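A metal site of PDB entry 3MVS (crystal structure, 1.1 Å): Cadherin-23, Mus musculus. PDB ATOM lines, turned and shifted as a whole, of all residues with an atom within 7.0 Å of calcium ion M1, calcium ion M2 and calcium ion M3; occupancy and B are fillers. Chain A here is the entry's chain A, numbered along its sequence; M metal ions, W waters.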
ATOM      1  N   GLU A  21      -6.987 -20.277  30.951  1.00  0.00           N
ATOM      2  CA  GLU A  21      -7.686 -19.024  30.711  1.00  0.00           C
ATOM      3  C   GLU A  21      -8.930 -19.176  29.832  1.00  0.00           C
ATOM      4  O   GLU A  21      -9.743 -18.258  29.787  1.00  0.00           O
ATOM      5  CB  GLU A  21      -6.763 -17.958  30.114  1.00  0.00           C
ATOM      6  CG  GLU A  21      -6.318 -18.252  28.677  1.00  0.00           C
ATOM      7  CD  GLU A  21      -5.488 -17.148  28.042  1.00  0.00           C
ATOM      8  OE1 GLU A  21      -5.690 -15.976  28.416  1.00  0.00           O
ATOM      9  OE2 GLU A  21      -4.681 -17.456  27.138  1.00  0.00           O
ATOM     10  N   LEU A  70     -10.570 -15.169  33.232  1.00  0.00           N
ATOM     11  CA  LEU A  70      -9.139 -15.106  33.483  1.00  0.00           C
ATOM     12  C   LEU A  70      -8.470 -14.723  32.173  1.00  0.00           C
ATOM     13  O   LEU A  70      -9.007 -14.995  31.104  1.00  0.00           O
ATOM     14  CB  LEU A  70      -8.609 -16.465  33.930  1.00  0.00           C
ATOM     15  CG  LEU A  70      -9.239 -17.006  35.208  1.00  0.00           C
ATOM     16  CD1 LEU A  70      -8.763 -18.425  35.431  1.00  0.00           C
ATOM     17  CD2 LEU A  70      -8.920 -16.125  36.393  1.00  0.00           C
ATOM     18  N   ASP A  71      -7.332 -14.054  32.259  1.00  0.00           N
ATOM     19  CA  ASP A  71      -6.627 -13.656  31.051  1.00  0.00           C
ATOM     20  C   ASP A  71      -5.152 -13.763  31.319  1.00  0.00           C
ATOM     21  O   ASP A  71      -4.588 -12.939  32.028  1.00  0.00           O
ATOM     22  CB  ASP A  71      -7.011 -12.241  30.627  1.00  0.00           C
ATOM     23  CG  ASP A  71      -6.276 -11.781  29.383  1.00  0.00           C
ATOM     24  OD1 ASP A  71      -5.704 -12.623  28.659  1.00  0.00           O
ATOM     25  OD2 ASP A  71      -6.275 -10.551  29.107  1.00  0.00           O
ATOM     26  N   ARG A  72      -4.526 -14.780  30.739  1.00  0.00           N
ATOM     27  CA  ARG A  72      -3.102 -15.014  30.915  1.00  0.00           C
ATOM     28  C   ARG A  72      -2.271 -13.814  30.488  1.00  0.00           C
ATOM     29  O   ARG A  72      -1.230 -13.511  31.079  1.00  0.00           O
ATOM     30  CB  ARG A  72      -2.675 -16.263  30.141  1.00  0.00           C
ATOM     31  CG  ARG A  72      -1.412 -16.979  30.629  1.00  0.00           C
ATOM     32  CD  ARG A  72      -0.090 -16.347  30.208  1.00  0.00           C
ATOM     33  NE  ARG A  72      -0.149 -15.884  28.828  1.00  0.00           N
ATOM     34  CZ  ARG A  72       0.747 -15.035  28.313  1.00  0.00           C
ATOM     35  NH1 ARG A  72       1.755 -14.610  29.064  1.00  0.00           N
ATOM     36  NH2 ARG A  72       0.643 -14.636  27.048  1.00  0.00           N
ATOM     37  N   GLU A  73      -2.765 -13.106  29.474  1.00  0.00           N
ATOM     38  CA  GLU A  73      -2.070 -11.917  28.935  1.00  0.00           C
ATOM     39  C   GLU A  73      -2.132 -10.692  29.850  1.00  0.00           C
ATOM     40  O   GLU A  73      -1.408  -9.713  29.614  1.00  0.00           O
ATOM     41  CB  GLU A  73      -2.626 -11.551  27.551  1.00  0.00           C
ATOM     42  CG  GLU A  73      -2.132 -12.385  26.380  1.00  0.00           C
ATOM     43  CD  GLU A  73      -2.686 -13.808  26.343  1.00  0.00           C
ATOM     44  OE1 GLU A  73      -3.901 -14.054  26.529  1.00  0.00           O
ATOM     45  OE2 GLU A  73      -1.888 -14.718  26.093  1.00  0.00           O
ATOM     46  N   THR A  74      -2.984 -10.730  30.873  1.00  0.00           N
ATOM     47  CA  THR A  74      -3.110  -9.638  31.849  1.00  0.00           C
ATOM     48  C   THR A  74      -2.449 -10.014  33.166  1.00  0.00           C
ATOM     49  O   THR A  74      -1.659  -9.241  33.717  1.00  0.00           O
ATOM     50  CB  THR A  74      -4.590  -9.253  32.094  1.00  0.00           C
ATOM     51  OG1 THR A  74      -5.173  -8.770  30.889  1.00  0.00           O
ATOM     52  CG2 THR A  74      -4.715  -8.193  33.180  1.00  0.00           C
ATOM     53  N   GLY A 100      -3.352 -20.746  32.915  1.00  0.00           N
ATOM     54  CA  GLY A 100      -2.748 -21.422  31.773  1.00  0.00           C
ATOM     55  C   GLY A 100      -3.053 -20.682  30.485  1.00  0.00           C
ATOM     56  O   GLY A 100      -4.170 -20.226  30.262  1.00  0.00           O
ATOM     57  N   ASP A 101      -2.053 -20.582  29.616  1.00  0.00           N
ATOM     58  CA  ASP A 101      -2.233 -19.893  28.341  1.00  0.00           C
ATOM     59  C   ASP A 101      -2.947 -20.786  27.349  1.00  0.00           C
ATOM     60  O   ASP A 101      -2.672 -21.975  27.260  1.00  0.00           O
ATOM     61  CB  ASP A 101      -0.882 -19.488  27.767  1.00  0.00           C
ATOM     62  CG  ASP A 101      -1.010 -18.581  26.544  1.00  0.00           C
ATOM     63  OD1 ASP A 101      -1.679 -17.547  26.647  1.00  0.00           O
ATOM     64  OD2 ASP A 101      -0.416 -18.875  25.481  1.00  0.00           O
ATOM     65  N   VAL A 102      -3.819 -20.171  26.555  1.00  0.00           N
ATOM     66  CA  VAL A 102      -4.280 -20.800  25.306  1.00  0.00           C
ATOM     67  C   VAL A 102      -4.044 -19.814  24.175  1.00  0.00           C
ATOM     68  O   VAL A 102      -3.791 -18.622  24.405  1.00  0.00           O
ATOM     69  CB  VAL A 102      -5.772 -21.258  25.339  1.00  0.00           C
ATOM     70  CG1 VAL A 102      -6.035 -22.146  26.534  1.00  0.00           C
ATOM     71  CG2 VAL A 102      -6.707 -20.067  25.314  1.00  0.00           C
ATOM     72  N   ASN A 103      -4.157 -20.282  22.938  1.00  0.00           N
ATOM     73  CA  ASN A 103      -4.029 -19.377  21.808  1.00  0.00           C
ATOM     74  C   ASN A 103      -5.358 -18.680  21.605  1.00  0.00           C
ATOM     75  O   ASN A 103      -6.267 -19.235  20.983  1.00  0.00           O
ATOM     76  CB  ASN A 103      -3.641 -20.115  20.532  1.00  0.00           C
ATOM     77  CG  ASN A 103      -3.290 -19.151  19.437  1.00  0.00           C
ATOM     78  OD1 ASN A 103      -2.557 -18.214  19.682  1.00  0.00           O
ATOM     79  ND2 ASN A 103      -3.807 -19.372  18.245  1.00  0.00           N
ATOM     80  N   ASP A 104      -5.480 -17.472  22.135  1.00  0.00           N
ATOM     81  CA  ASP A 104      -6.741 -16.724  22.075  1.00  0.00           C
ATOM     82  C   ASP A 104      -6.607 -15.314  21.515  1.00  0.00           C
ATOM     83  O   ASP A 104      -7.551 -14.528  21.551  1.00  0.00           O
ATOM     84  CB  ASP A 104      -7.486 -16.733  23.428  1.00  0.00           C
ATOM     85  CG  ASP A 104      -6.703 -16.095  24.581  1.00  0.00           C
ATOM     86  OD1 ASP A 104      -5.483 -15.856  24.478  1.00  0.00           O
ATOM     87  OD2 ASP A 104      -7.321 -15.794  25.632  1.00  0.00           O
ATOM     88  N   ASN A 105      -5.435 -15.020  20.966  1.00  0.00           N
ATOM     89  CA  ASN A 105      -5.209 -13.749  20.267  1.00  0.00           C
ATOM     90  C   ASN A 105      -4.805 -14.035  18.834  1.00  0.00           C
ATOM     91  O   ASN A 105      -4.005 -14.911  18.571  1.00  0.00           O
ATOM     92  CB  ASN A 105      -4.082 -12.922  20.903  1.00  0.00           C
ATOM     93  CG  ASN A 105      -4.441 -12.427  22.280  1.00  0.00           C
ATOM     94  OD1 ASN A 105      -4.889 -11.288  22.450  1.00  0.00           O
ATOM     95  ND2 ASN A 105      -4.288 -13.297  23.279  1.00  0.00           N
ATOM     96  N   ALA A 106      -5.395 -13.299  17.900  1.00  0.00           N
ATOM     97  CA  ALA A 106      -4.875 -13.269  16.535  1.00  0.00           C
ATOM     98  C   ALA A 106      -3.785 -12.203  16.457  1.00  0.00           C
ATOM     99  O   ALA A 106      -3.693 -11.338  17.330  1.00  0.00           O
ATOM    100  CB  ALA A 106      -6.013 -12.947  15.563  1.00  0.00           C
ATOM    101  N   PRO A 107      -2.966 -12.224  15.397  1.00  0.00           N
ATOM    102  CA  PRO A 107      -1.921 -11.189  15.261  1.00  0.00           C
ATOM    103  C   PRO A 107      -2.492  -9.778  15.076  1.00  0.00           C
ATOM    104  O   PRO A 107      -3.581  -9.611  14.534  1.00  0.00           O
ATOM    105  CB  PRO A 107      -1.135 -11.648  14.022  1.00  0.00           C
ATOM    106  CG  PRO A 107      -1.352 -13.139  14.006  1.00  0.00           C
ATOM    107  CD  PRO A 107      -2.776 -13.320  14.422  1.00  0.00           C
ATOM    108  N   ASP A 135       1.969 -10.927  18.229  1.00  0.00           N
ATOM    109  CA  ASP A 135       0.943 -11.778  18.804  1.00  0.00           C
ATOM    110  C   ASP A 135       1.400 -12.158  20.215  1.00  0.00           C
ATOM    111  O   ASP A 135       2.504 -12.682  20.370  1.00  0.00           O
ATOM    112  CB  ASP A 135       0.799 -13.015  17.916  1.00  0.00           C
ATOM    113  CG  ASP A 135      -0.363 -13.904  18.298  1.00  0.00           C
ATOM    114  OD1 ASP A 135      -0.581 -14.178  19.499  1.00  0.00           O
ATOM    115  OD2 ASP A 135      -1.056 -14.408  17.377  1.00  0.00           O
ATOM    116  N   PRO A 136       0.575 -11.912  21.249  1.00  0.00           N
ATOM    117  CA  PRO A 136       1.053 -12.044  22.641  1.00  0.00           C
ATOM    118  C   PRO A 136       0.928 -13.440  23.224  1.00  0.00           C
ATOM    119  O   PRO A 136       1.368 -13.659  24.358  1.00  0.00           O
ATOM    120  CB  PRO A 136       0.123 -11.108  23.400  1.00  0.00           C
ATOM    121  CG  PRO A 136      -1.170 -11.226  22.675  1.00  0.00           C
ATOM    122  CD  PRO A 136      -0.747 -11.276  21.189  1.00  0.00           C
ATOM    123  N   ASP A 137       0.315 -14.389  22.520  1.00  0.00           N
ATOM    124  CA  ASP A 137       0.200 -15.735  23.047  1.00  0.00           C
ATOM    125  C   ASP A 137       1.562 -16.382  23.168  1.00  0.00           C
ATOM    126  O   ASP A 137       2.501 -15.979  22.481  1.00  0.00           O
ATOM    127  CB  ASP A 137      -0.729 -16.596  22.192  1.00  0.00           C
ATOM    128  CG  ASP A 137      -2.155 -16.084  22.196  1.00  0.00           C
ATOM    129  OD1 ASP A 137      -2.740 -15.944  23.292  1.00  0.00           O
ATOM    130  OD2 ASP A 137      -2.675 -15.792  21.105  1.00  0.00           O
ATOM    131  N   LEU A 138       1.676 -17.381  24.017  1.00  0.00           N
ATOM    132  CA  LEU A 138       2.952 -18.010  24.254  1.00  0.00           C
ATOM    133  C   LEU A 138       3.283 -19.037  23.190  1.00  0.00           C
ATOM    134  O   LEU A 138       2.375 -19.587  22.538  1.00  0.00           O
ATOM    135  CB  LEU A 138       2.987 -18.659  25.647  1.00  0.00           C
ATOM    136  CG  LEU A 138       2.741 -17.698  26.798  1.00  0.00           C
ATOM    137  CD1 LEU A 138       2.854 -18.416  28.139  1.00  0.00           C
ATOM    138  CD2 LEU A 138       3.722 -16.511  26.753  1.00  0.00           C
ATOM    139  N   ALA A 140       4.183 -21.305  20.052  1.00  0.00           N
ATOM    140  CA  ALA A 140       3.828 -21.290  18.636  1.00  0.00           C
ATOM    141  C   ALA A 140       2.642 -20.379  18.347  1.00  0.00           C
ATOM    142  O   ALA A 140       2.558 -19.792  17.275  1.00  0.00           O
ATOM    143  CB  ALA A 140       3.557 -22.699  18.140  1.00  0.00           C
ATOM    144  N   GLY A 141       1.754 -20.225  19.333  1.00  0.00           N
ATOM    145  CA  GLY A 141       0.638 -19.315  19.185  1.00  0.00           C
ATOM    146  C   GLY A 141       1.009 -17.850  19.105  1.00  0.00           C
ATOM    147  O   GLY A 141       0.152 -17.032  18.757  1.00  0.00           O
ATOM    148  N   GLY A 142       2.264 -17.502  19.428  1.00  0.00           N
ATOM    149  CA  GLY A 142       2.748 -16.128  19.312  1.00  0.00           C
ATOM    150  C   GLY A 142       3.655 -15.903  18.116  1.00  0.00           C
ATOM    151  O   GLY A 142       4.133 -14.793  17.913  1.00  0.00           O
ATOM    152  N   SER A 143       3.888 -16.975  17.350  1.00  0.00           N
ATOM    153  CA  SER A 143       4.743 -16.919  16.170  1.00  0.00           C
ATOM    154  C   SER A 143       3.896 -16.672  14.929  1.00  0.00           C
ATOM    155  O   SER A 143       2.940 -17.392  14.678  1.00  0.00           O
ATOM    156  CB  SER A 143       5.511 -18.237  16.018  1.00  0.00           C
ATOM    157  OG  SER A 143       6.314 -18.225  14.863  1.00  0.00           O
ATOM    158  N   VAL A 144       4.271 -15.661  14.161  1.00  0.00           N
ATOM    159  CA  VAL A 144       3.460 -15.174  13.037  1.00  0.00           C
ATOM    160  C   VAL A 144       4.117 -15.492  11.701  1.00  0.00           C
ATOM    161  O   VAL A 144       5.328 -15.289  11.527  1.00  0.00           O
ATOM    162  CB  VAL A 144       3.297 -13.632  13.171  1.00  0.00           C
ATOM    163  CG1 VAL A 144       2.487 -13.072  11.989  1.00  0.00           C
ATOM    164  CG2 VAL A 144       2.619 -13.275  14.490  1.00  0.00           C
ATOM    165  N   ASP A 186      -0.925 -17.107  13.124  1.00  0.00           N
ATOM    166  CA  ASP A 186      -0.038 -17.687  14.105  1.00  0.00           C
ATOM    167  C   ASP A 186       0.124 -19.182  13.887  1.00  0.00           C
ATOM    168  O   ASP A 186      -0.519 -19.783  13.033  1.00  0.00           O
ATOM    169  CB  ASP A 186      -0.445 -17.277  15.539  1.00  0.00           C
ATOM    170  CG  ASP A 186      -1.755 -17.885  15.984  1.00  0.00           C
ATOM    171  OD1 ASP A 186      -2.093 -18.995  15.531  1.00  0.00           O
ATOM    172  OD2 ASP A 186      -2.449 -17.267  16.826  1.00  0.00           O
ATOM    173  N   GLN A 187       1.018 -19.796  14.652  1.00  0.00           N
ATOM    174  CA  GLN A 187       1.454 -21.160  14.363  1.00  0.00           C
ATOM    175  C   GLN A 187       0.986 -22.180  15.394  1.00  0.00           C
ATOM    176  O   GLN A 187       1.543 -23.280  15.491  1.00  0.00           O
ATOM    177  CB  GLN A 187       2.972 -21.197  14.163  1.00  0.00           C
ATOM    178  CG  GLN A 187       3.429 -20.307  13.005  1.00  0.00           C
ATOM    179  CD  GLN A 187       2.774 -20.696  11.705  1.00  0.00           C
ATOM    180  OE1 GLN A 187       2.010 -19.926  11.123  1.00  0.00           O
ATOM    181  NE2 GLN A 187       3.068 -21.901  11.241  1.00  0.00           N
ATOM    182  N   ASP A 188      -0.045 -21.838  16.159  1.00  0.00           N
ATOM    183  CA  ASP A 188      -0.600 -22.811  17.100  1.00  0.00           C
ATOM    184  C   ASP A 188      -1.024 -24.073  16.343  1.00  0.00           C
ATOM    185  O   ASP A 188      -1.634 -23.996  15.278  1.00  0.00           O
ATOM    186  CB  ASP A 188      -1.807 -22.237  17.839  1.00  0.00           C
ATOM    187  CG  ASP A 188      -2.264 -23.149  18.947  1.00  0.00           C
ATOM    188  OD1 ASP A 188      -1.662 -23.114  20.033  1.00  0.00           O
ATOM    189  OD2 ASP A 188      -3.210 -23.928  18.721  1.00  0.00           O
ATOM    190  N   ARG A 191      -5.289 -24.707  17.127  1.00  0.00           N
ATOM    191  CA  ARG A 191      -6.238 -23.660  16.780  1.00  0.00           C
ATOM    192  C   ARG A 191      -5.540 -22.358  16.355  1.00  0.00           C
ATOM    193  O   ARG A 191      -5.584 -21.351  17.079  1.00  0.00           O
ATOM    194  CB  ARG A 191      -7.222 -23.419  17.915  1.00  0.00           C
ATOM    195  CG  ARG A 191      -8.641 -23.221  17.427  1.00  0.00           C
ATOM    196  N   PRO A 192      -4.922 -22.374  15.174  1.00  0.00           N
ATOM    197  CA  PRO A 192      -4.283 -21.161  14.679  1.00  0.00           C
ATOM    198  C   PRO A 192      -5.293 -20.041  14.402  1.00  0.00           C
ATOM    199  O   PRO A 192      -6.442 -20.329  14.019  1.00  0.00           O
ATOM    200  CB  PRO A 192      -3.583 -21.614  13.404  1.00  0.00           C
ATOM    201  CG  PRO A 192      -4.353 -22.816  12.951  1.00  0.00           C
ATOM    202  CD  PRO A 192      -4.783 -23.482  14.212  1.00  0.00           C
ATOM    203  N   LEU A 193      -4.854 -18.799  14.589  1.00  0.00           N
ATOM    204  CA  LEU A 193      -5.688 -17.630  14.399  1.00  0.00           C
ATOM    205  C   LEU A 193      -5.073 -16.679  13.393  1.00  0.00           C
ATOM    206  O   LEU A 193      -3.847 -16.535  13.349  1.00  0.00           O
ATOM    207  CB  LEU A 193      -5.903 -16.930  15.731  1.00  0.00           C
ATOM    208  CG  LEU A 193      -6.691 -17.744  16.761  1.00  0.00           C
ATOM    209  CD1 LEU A 193      -6.717 -16.980  18.085  1.00  0.00           C
ATOM    210  CD2 LEU A 193      -8.114 -18.023  16.324  1.00  0.00           C
HETATM  211 CA    CA M   1      -1.994 -16.099  18.808  1.00  0.00          CA
HETATM  212 CA    CA M   2      -3.361 -16.520  25.451  1.00  0.00          CA
HETATM  213 CA    CA M   3      -6.182 -14.188  26.981  1.00  0.00          CA
HETATM  214  O   HOH W   1      -8.359 -13.742  27.658  1.00  0.00           O
HETATM  215  O   HOH W   2      -6.401 -12.480  25.377  1.00  0.00           O
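Calcium ion M2 is bound by OD1 of Asp 101 (2.3 Å), OD1 of Asp 137 (2.3 Å), OE2 of Glu 21 (2.3 Å), O of Val 102 (2.4 Å), OE2 of Glu 73 (2.4 Å), OD1 of Asp 104 (2.4 Å) and OE1 of Glu 73 (2.7 Å).
Calcium ion M2 has seven donor atoms within binding distance.
Of the 29 residues printed, 4 come within 4 Å of calcium ion M3.
Calcium ion M1 is bound by O of Gly 141, OD2 of Asp 186, O of Asn 105, OD1 of Asn 103, OD2 of Asp 135, OD2 of Asp 137 and OD1 of Asp 135.
Calcium ion M1 has seven donor atoms within binding distance.
OD1 of Asp 101 sits close to NE of Arg 72 (3.1 Å).
The side-chain carboxylate (OD2) of Asp 101 is in hydrogen-bond range of the backbone NH (N) of Leu 138.
The backbone carbonyl oxygen (O) of Asp 137 lies close to the backbone NH (N) of Gly 142 (3.4 Å).
The side-chain carboxylate (OE1) of Glu 73 sits close to the side-chain amide nitrogen (ND2) of Asn 105, 3.4 Å away.
OE2 of Glu 73 sits close to NH2 of Arg 72 (2.7 Å).
The backbone NH (N) of Arg 72 sits close to the side-chain carboxylate (OE1) of Glu 21, at 2.9 Å.
OD2 of Asp 71 is in hydrogen-bond range of OG1 of Thr 74 (2.7 Å).
The side-chain carboxylate (OD1) of Asp 186 is in hydrogen-bond range of the backbone NH (N) of Leu 193.
Six residues have an atom within 4 Å of calcium ion M1: Asn 103, Asn 105, Asp 135, Asp 137, Gly 141 and Asp 186.
Calcium ion M3 is bound by water W1 (2.3 Å), OE1 of Glu 73 (2.3 Å), OD1 of Asp 71 (2.3 Å), OE1 of Glu 21 (2.3 Å), water W2 (2.4 Å) and OD2 of Asp 104 (2.4 Å).
Calcium ion M3 has six donor atoms within binding distance.
Slightly farther from calcium ion M3 lies the side-chain carboxylate (OD1) of Asp 104 (3.1 Å).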
